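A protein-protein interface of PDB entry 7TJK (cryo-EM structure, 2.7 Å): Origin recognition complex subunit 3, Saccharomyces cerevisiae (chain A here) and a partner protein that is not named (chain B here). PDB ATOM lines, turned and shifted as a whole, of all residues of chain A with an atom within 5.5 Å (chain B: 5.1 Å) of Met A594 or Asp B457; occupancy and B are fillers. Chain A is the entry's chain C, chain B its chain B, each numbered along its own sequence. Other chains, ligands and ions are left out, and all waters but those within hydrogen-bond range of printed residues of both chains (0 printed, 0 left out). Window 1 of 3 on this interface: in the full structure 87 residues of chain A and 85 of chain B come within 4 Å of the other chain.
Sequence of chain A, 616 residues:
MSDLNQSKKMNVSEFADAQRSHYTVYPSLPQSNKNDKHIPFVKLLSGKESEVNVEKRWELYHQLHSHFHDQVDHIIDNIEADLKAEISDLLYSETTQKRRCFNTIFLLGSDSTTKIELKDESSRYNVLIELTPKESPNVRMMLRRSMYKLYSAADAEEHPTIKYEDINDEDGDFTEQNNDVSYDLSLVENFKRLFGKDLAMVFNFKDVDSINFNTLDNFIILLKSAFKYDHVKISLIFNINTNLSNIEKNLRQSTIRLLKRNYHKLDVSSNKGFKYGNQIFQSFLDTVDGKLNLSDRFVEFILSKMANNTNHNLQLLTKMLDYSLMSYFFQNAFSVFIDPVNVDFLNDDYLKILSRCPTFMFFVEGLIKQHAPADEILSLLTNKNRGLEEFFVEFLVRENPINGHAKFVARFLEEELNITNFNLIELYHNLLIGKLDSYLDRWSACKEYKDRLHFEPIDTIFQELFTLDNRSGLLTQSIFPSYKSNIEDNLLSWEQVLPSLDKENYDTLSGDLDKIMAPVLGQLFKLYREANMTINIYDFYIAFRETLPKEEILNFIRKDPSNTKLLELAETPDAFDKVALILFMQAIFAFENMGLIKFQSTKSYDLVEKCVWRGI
Among the printed residues, pairs that only touch across the chains: Tyr A483 with Ile B459 (3.2 Å), Ile A487 with Gly B318 (3.7 Å), Ile A487 with Ile B459 (3.8 Å), Leu A491 with Val B319 (3.7 Å), Asn A593 with His B458 (3.99 Å), Met A594 with Asp B457 (3.7 Å), Met A594 with His B458 (3.4 Å), Gly A595 with His B458 (3.7 Å) and Leu A596 with Ile B459 (3.8 Å).
The side-chain hydroxyl (OG1) of Thr B456 lies close to the side-chain hydroxyl (OH) of Tyr A483 (3.4 Å).
O of His B458 sits at hydrogen-bond distance from OH of Tyr A483.
The backbone NH (N) of Ile B459 lies within hydrogen-bond range of the backbone carbonyl oxygen (O) of Met A594 (3.1 Å).
Hydrophobic or aromatic side chains of chain B that line the printed part of chain A: Val B319, His B458 and Ile B459.
Along chain B the printed residues that touch a printed residue of chain A span positions 318 to 459.
Of the 11 printed residues of chain A, 7 touch a printed residue of chain B.
Among the printed residues, 12 pairs touch across the chains.
Among the printed residues, no Asp or Glu carboxylate lies within 4 Å of a Lys or Arg side-chain nitrogen of the other chain.
OD1 of Asp B457 lies within salt-bridge range of NZ of Lys B322 (3.0 Å).
OD1 of Asn B426 lies close to OD2 of Asp B457.
OG1 of Thr B456 lies within hydrogen-bond range of OD2 of Asp B428.
The side-chain carboxylate (OD2) of Asp B428 is in hydrogen-bond range of the backbone NH (N) of Asp B457, at 2.6 Å.
The backbone NH (N) of His B458 sits at hydrogen-bond distance from the side-chain carboxylate (OD2) of Asp B428 (2.4 Å).
The backbone carbonyl oxygen (O) of Phe A591 lies within hydrogen-bond range of the backbone NH (N) of Leu A596, 2.9 Å away.
Phe A591 touches none of the printed residues of chain B.
Printed residues of chain B within 4 Å of Asn A593: His B458 (3.99 Å).
Met A594 touches just these residues of chain B: Asp B457 (3.7 Å), His B458 (3.4 Å) and Ile B459 (3.1 Å).
Asn B426 touches none of the printed residues of chain A.
Of the printed residues of chain A, Thr B456 touches Tyr A483 (3.3 Å).
Asp B457 touches just one residue of chain A: Met A594 (3.7 Å).
The nearest residue of chain B that does not touch Met A594 is Val B319 (4.1 Å).
The nearest residue of chain A that does not touch Asp B457 is Tyr A483 (4.4 Å).
The nearest printed residue of chain A that does not touch Ile B459 is Gly A595 (4.6 Å).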
ATOM      1  N   TYR A 483      -0.280 -16.733   1.079  1.00  0.00           N
ATOM      2  CA  TYR A 483      -1.178 -17.093  -0.020  1.00  0.00           C
ATOM      3  C   TYR A 483      -1.795 -15.868  -0.690  1.00  0.00           C
ATOM      4  O   TYR A 483      -1.671 -15.681  -1.908  1.00  0.00           O
ATOM      5  CB  TYR A 483      -2.255 -18.035   0.548  1.00  0.00           C
ATOM      6  CG  TYR A 483      -3.424 -18.420  -0.341  1.00  0.00           C
ATOM      7  CD1 TYR A 483      -4.572 -17.630  -0.413  1.00  0.00           C
ATOM      8  CD2 TYR A 483      -3.407 -19.607  -1.057  1.00  0.00           C
ATOM      9  CE1 TYR A 483      -5.638 -17.987  -1.208  1.00  0.00           C
ATOM     10  CE2 TYR A 483      -4.479 -19.976  -1.846  1.00  0.00           C
ATOM     11  CZ  TYR A 483      -5.587 -19.162  -1.921  1.00  0.00           C
ATOM     12  OH  TYR A 483      -6.655 -19.521  -2.708  1.00  0.00           O
ATOM     13  N   ILE A 487      -0.800 -14.112  -4.311  1.00  0.00           N
ATOM     14  CA  ILE A 487      -1.740 -13.738  -5.370  1.00  0.00           C
ATOM     15  C   ILE A 487      -1.573 -12.267  -5.745  1.00  0.00           C
ATOM     16  O   ILE A 487      -1.550 -11.911  -6.932  1.00  0.00           O
ATOM     17  CB  ILE A 487      -3.184 -14.051  -4.934  1.00  0.00           C
ATOM     18  CG1 ILE A 487      -3.366 -15.551  -4.709  1.00  0.00           C
ATOM     19  CG2 ILE A 487      -4.186 -13.568  -5.970  1.00  0.00           C
ATOM     20  CD1 ILE A 487      -3.039 -16.386  -5.911  1.00  0.00           C
ATOM     21  N   LEU A 491      -0.297 -10.766  -9.316  1.00  0.00           N
ATOM     22  CA  LEU A 491      -1.173  -9.926 -10.128  1.00  0.00           C
ATOM     23  C   LEU A 491      -0.552  -8.563 -10.411  1.00  0.00           C
ATOM     24  O   LEU A 491      -0.723  -8.018 -11.507  1.00  0.00           O
ATOM     25  CB  LEU A 491      -2.526  -9.761  -9.439  1.00  0.00           C
ATOM     26  CG  LEU A 491      -3.568 -10.824  -9.777  1.00  0.00           C
ATOM     27  CD1 LEU A 491      -4.823 -10.623  -8.953  1.00  0.00           C
ATOM     28  CD2 LEU A 491      -3.881 -10.762 -11.259  1.00  0.00           C
ATOM     29  N   PHE A 589     -15.408 -10.618 -14.334  1.00  0.00           N
ATOM     30  CA  PHE A 589     -15.967 -11.840 -13.758  1.00  0.00           C
ATOM     31  C   PHE A 589     -14.896 -12.796 -13.246  1.00  0.00           C
ATOM     32  O   PHE A 589     -15.164 -13.551 -12.302  1.00  0.00           O
ATOM     33  CB  PHE A 589     -16.901 -12.549 -14.743  1.00  0.00           C
ATOM     34  CG  PHE A 589     -18.227 -11.857 -14.929  1.00  0.00           C
ATOM     35  CD1 PHE A 589     -18.384 -10.826 -15.837  1.00  0.00           C
ATOM     36  CD2 PHE A 589     -19.322 -12.246 -14.170  1.00  0.00           C
ATOM     37  CE1 PHE A 589     -19.608 -10.196 -15.995  1.00  0.00           C
ATOM     38  CE2 PHE A 589     -20.548 -11.622 -14.319  1.00  0.00           C
ATOM     39  CZ  PHE A 589     -20.690 -10.595 -15.233  1.00  0.00           C
ATOM     40  N   ALA A 590     -13.680 -12.762 -13.807  1.00  0.00           N
ATOM     41  CA  ALA A 590     -12.575 -13.497 -13.191  1.00  0.00           C
ATOM     42  C   ALA A 590     -12.241 -12.945 -11.808  1.00  0.00           C
ATOM     43  O   ALA A 590     -12.020 -13.715 -10.865  1.00  0.00           O
ATOM     44  CB  ALA A 590     -11.347 -13.454 -14.099  1.00  0.00           C
ATOM     45  N   PHE A 591     -12.225 -11.614 -11.669  1.00  0.00           N
ATOM     46  CA  PHE A 591     -11.977 -10.973 -10.377  1.00  0.00           C
ATOM     47  C   PHE A 591     -13.091 -11.281  -9.382  1.00  0.00           C
ATOM     48  O   PHE A 591     -12.835 -11.447  -8.185  1.00  0.00           O
ATOM     49  CB  PHE A 591     -11.843  -9.458 -10.558  1.00  0.00           C
ATOM     50  CG  PHE A 591     -10.452  -8.988 -10.912  1.00  0.00           C
ATOM     51  CD1 PHE A 591      -9.573  -9.797 -11.619  1.00  0.00           C
ATOM     52  CD2 PHE A 591     -10.036  -7.718 -10.546  1.00  0.00           C
ATOM     53  CE1 PHE A 591      -8.307  -9.353 -11.942  1.00  0.00           C
ATOM     54  CE2 PHE A 591      -8.770  -7.267 -10.865  1.00  0.00           C
ATOM     55  CZ  PHE A 591      -7.905  -8.086 -11.564  1.00  0.00           C
ATOM     56  N   GLU A 592     -14.333 -11.339  -9.865  1.00  0.00           N
ATOM     57  CA  GLU A 592     -15.471 -11.730  -9.042  1.00  0.00           C
ATOM     58  C   GLU A 592     -15.378 -13.179  -8.582  1.00  0.00           C
ATOM     59  O   GLU A 592     -15.745 -13.481  -7.441  1.00  0.00           O
ATOM     60  CB  GLU A 592     -16.773 -11.505  -9.820  1.00  0.00           C
ATOM     61  CG  GLU A 592     -18.061 -11.831  -9.063  1.00  0.00           C
ATOM     62  CD  GLU A 592     -18.312 -10.927  -7.869  1.00  0.00           C
ATOM     63  OE1 GLU A 592     -17.822  -9.777  -7.864  1.00  0.00           O
ATOM     64  OE2 GLU A 592     -19.004 -11.370  -6.929  1.00  0.00           O
ATOM     65  N   ASN A 593     -14.897 -14.078  -9.440  1.00  0.00           N
ATOM     66  CA  ASN A 593     -14.691 -15.465  -9.046  1.00  0.00           C
ATOM     67  C   ASN A 593     -13.559 -15.628  -8.039  1.00  0.00           C
ATOM     68  O   ASN A 593     -13.677 -16.445  -7.117  1.00  0.00           O
ATOM     69  CB  ASN A 593     -14.410 -16.328 -10.277  1.00  0.00           C
ATOM     70  CG  ASN A 593     -14.925 -17.743 -10.123  1.00  0.00           C
ATOM     71  OD1 ASN A 593     -15.595 -18.067  -9.142  1.00  0.00           O
ATOM     72  ND2 ASN A 593     -14.616 -18.596 -11.092  1.00  0.00           N
ATOM     73  N   MET A 594     -12.467 -14.870  -8.185  1.00  0.00           N
ATOM     74  CA  MET A 594     -11.409 -14.902  -7.179  1.00  0.00           C
ATOM     75  C   MET A 594     -11.812 -14.217  -5.879  1.00  0.00           C
ATOM     76  O   MET A 594     -11.204 -14.489  -4.840  1.00  0.00           O
ATOM     77  CB  MET A 594     -10.129 -14.260  -7.711  1.00  0.00           C
ATOM     78  CG  MET A 594      -9.622 -14.848  -9.008  1.00  0.00           C
ATOM     79  SD  MET A 594      -8.195 -13.958  -9.651  1.00  0.00           S
ATOM     80  CE  MET A 594      -7.027 -14.213  -8.326  1.00  0.00           C
ATOM     81  N   GLY A 595     -12.813 -13.343  -5.910  1.00  0.00           N
ATOM     82  CA  GLY A 595     -13.250 -12.668  -4.708  1.00  0.00           C
ATOM     83  C   GLY A 595     -12.612 -11.322  -4.460  1.00  0.00           C
ATOM     84  O   GLY A 595     -12.710 -10.800  -3.342  1.00  0.00           O
ATOM     85  N   LEU A 596     -11.952 -10.743  -5.462  1.00  0.00           N
ATOM     86  CA  LEU A 596     -11.367  -9.416  -5.319  1.00  0.00           C
ATOM     87  C   LEU A 596     -12.416  -8.311  -5.290  1.00  0.00           C
ATOM     88  O   LEU A 596     -12.259  -7.341  -4.540  1.00  0.00           O
ATOM     89  CB  LEU A 596     -10.376  -9.146  -6.455  1.00  0.00           C
ATOM     90  CG  LEU A 596      -9.324 -10.215  -6.760  1.00  0.00           C
ATOM     91  CD1 LEU A 596      -8.496  -9.824  -7.972  1.00  0.00           C
ATOM     92  CD2 LEU A 596      -8.425 -10.452  -5.567  1.00  0.00           C
ATOM     93  N   GLY B 318      -2.865 -19.939  -7.390  1.00  0.00           N
ATOM     94  CA  GLY B 318      -2.308 -19.037  -8.374  1.00  0.00           C
ATOM     95  C   GLY B 318      -3.386 -18.407  -9.223  1.00  0.00           C
ATOM     96  O   GLY B 318      -4.501 -18.928  -9.303  1.00  0.00           O
ATOM     97  N   VAL B 319      -3.075 -17.280  -9.853  1.00  0.00           N
ATOM     98  CA  VAL B 319      -4.004 -16.596 -10.742  1.00  0.00           C
ATOM     99  C   VAL B 319      -4.056 -17.362 -12.061  1.00  0.00           C
ATOM    100  O   VAL B 319      -3.028 -17.845 -12.557  1.00  0.00           O
ATOM    101  CB  VAL B 319      -3.621 -15.112 -10.919  1.00  0.00           C
ATOM    102  CG1 VAL B 319      -2.224 -14.927 -11.515  1.00  0.00           C
ATOM    103  CG2 VAL B 319      -4.669 -14.370 -11.742  1.00  0.00           C
ATOM    104  N   GLY B 320      -5.259 -17.546 -12.584  1.00  0.00           N
ATOM    105  CA  GLY B 320      -5.483 -18.353 -13.764  1.00  0.00           C
ATOM    106  C   GLY B 320      -6.064 -19.713 -13.415  1.00  0.00           C
ATOM    107  O   GLY B 320      -6.027 -20.172 -12.272  1.00  0.00           O
ATOM    108  N   LYS B 322      -6.530 -23.810 -13.409  1.00  0.00           N
ATOM    109  CA  LYS B 322      -5.618 -24.919 -13.164  1.00  0.00           C
ATOM    110  C   LYS B 322      -6.226 -26.263 -13.539  1.00  0.00           C
ATOM    111  O   LYS B 322      -5.764 -27.296 -13.050  1.00  0.00           O
ATOM    112  CB  LYS B 322      -5.174 -24.935 -11.702  1.00  0.00           C
ATOM    113  CG  LYS B 322      -4.296 -23.767 -11.317  1.00  0.00           C
ATOM    114  CD  LYS B 322      -4.407 -23.458  -9.845  1.00  0.00           C
ATOM    115  CE  LYS B 322      -5.693 -22.723  -9.565  1.00  0.00           C
ATOM    116  NZ  LYS B 322      -5.657 -21.311 -10.028  1.00  0.00           N
ATOM    117  N   ASN B 426     -11.260 -26.832  -8.188  1.00  0.00           N
ATOM    118  CA  ASN B 426     -11.960 -25.723  -7.533  1.00  0.00           C
ATOM    119  C   ASN B 426     -12.602 -26.163  -6.212  1.00  0.00           C
ATOM    120  O   ASN B 426     -13.822 -26.236  -6.073  1.00  0.00           O
ATOM    121  CB  ASN B 426     -12.994 -25.087  -8.471  1.00  0.00           C
ATOM    122  CG  ASN B 426     -12.410 -23.968  -9.300  1.00  0.00           C
ATOM    123  OD1 ASN B 426     -12.436 -22.807  -8.897  1.00  0.00           O
ATOM    124  ND2 ASN B 426     -11.878 -24.309 -10.467  1.00  0.00           N
ATOM    125  N   ASP B 428     -12.811 -24.503  -3.618  1.00  0.00           N
ATOM    126  CA  ASP B 428     -13.509 -23.372  -3.030  1.00  0.00           C
ATOM    127  C   ASP B 428     -14.730 -22.937  -3.834  1.00  0.00           C
ATOM    128  O   ASP B 428     -15.228 -21.828  -3.622  1.00  0.00           O
ATOM    129  CB  ASP B 428     -12.543 -22.202  -2.895  1.00  0.00           C
ATOM    130  CG  ASP B 428     -11.717 -21.996  -4.140  1.00  0.00           C
ATOM    131  OD1 ASP B 428     -11.900 -22.747  -5.119  1.00  0.00           O
ATOM    132  OD2 ASP B 428     -10.858 -21.096  -4.134  1.00  0.00           O
ATOM    133  N   SER B 455      -7.241 -27.940  -6.266  1.00  0.00           N
ATOM    134  CA  SER B 455      -6.924 -26.582  -6.675  1.00  0.00           C
ATOM    135  C   SER B 455      -7.860 -25.619  -5.961  1.00  0.00           C
ATOM    136  O   SER B 455      -8.840 -26.028  -5.338  1.00  0.00           O
ATOM    137  CB  SER B 455      -7.033 -26.404  -8.195  1.00  0.00           C
ATOM    138  OG  SER B 455      -8.388 -26.331  -8.605  1.00  0.00           O
ATOM    139  N   THR B 456      -7.546 -24.329  -6.053  1.00  0.00           N
ATOM    140  CA  THR B 456      -8.341 -23.284  -5.423  1.00  0.00           C
ATOM    141  C   THR B 456      -8.202 -21.974  -6.189  1.00  0.00           C
ATOM    142  O   THR B 456      -7.196 -21.740  -6.865  1.00  0.00           O
ATOM    143  CB  THR B 456      -7.935 -23.093  -3.952  1.00  0.00           C
ATOM    144  OG1 THR B 456      -8.777 -22.115  -3.344  1.00  0.00           O
ATOM    145  CG2 THR B 456      -6.507 -22.648  -3.830  1.00  0.00           C
ATOM    146  N   ASP B 457      -9.223 -21.128  -6.093  1.00  0.00           N
ATOM    147  CA  ASP B 457      -9.246 -19.851  -6.798  1.00  0.00           C
ATOM    148  C   ASP B 457      -9.551 -18.664  -5.902  1.00  0.00           C
ATOM    149  O   ASP B 457      -9.084 -17.557  -6.179  1.00  0.00           O
ATOM    150  CB  ASP B 457     -10.270 -19.891  -7.937  1.00  0.00           C
ATOM    151  CG  ASP B 457      -9.686 -20.430  -9.225  1.00  0.00           C
ATOM    152  OD1 ASP B 457      -8.459 -20.300  -9.422  1.00  0.00           O
ATOM    153  OD2 ASP B 457     -10.451 -20.976 -10.045  1.00  0.00           O
ATOM    154  N   HIS B 458     -10.333 -18.860  -4.843  1.00  0.00           N
ATOM    155  CA  HIS B 458     -10.691 -17.757  -3.962  1.00  0.00           C
ATOM    156  C   HIS B 458      -9.501 -17.345  -3.106  1.00  0.00           C
ATOM    157  O   HIS B 458      -8.740 -18.181  -2.611  1.00  0.00           O
ATOM    158  CB  HIS B 458     -11.873 -18.146  -3.073  1.00  0.00           C
ATOM    159  CG  HIS B 458     -12.693 -16.983  -2.616  1.00  0.00           C
ATOM    160  ND1 HIS B 458     -12.378 -16.245  -1.496  1.00  0.00           N
ATOM    161  CD2 HIS B 458     -13.810 -16.423  -3.134  1.00  0.00           C
ATOM    162  CE1 HIS B 458     -13.269 -15.284  -1.341  1.00  0.00           C
ATOM    163  NE2 HIS B 458     -14.148 -15.369  -2.322  1.00  0.00           N
ATOM    164  N   ILE B 459      -9.346 -16.031  -2.934  1.00  0.00           N
ATOM    165  CA  ILE B 459      -8.207 -15.497  -2.195  1.00  0.00           C
ATOM    166  C   ILE B 459      -8.372 -15.682  -0.687  1.00  0.00           C
ATOM    167  O   ILE B 459      -7.389 -15.580   0.058  1.00  0.00           O
ATOM    168  CB  ILE B 459      -8.008 -14.020  -2.592  1.00  0.00           C
ATOM    169  CG1 ILE B 459      -6.579 -13.545  -2.304  1.00  0.00           C
ATOM    170  CG2 ILE B 459      -9.022 -13.127  -1.898  1.00  0.00           C
ATOM    171  CD1 ILE B 459      -6.199 -12.281  -3.029  1.00  0.00           C
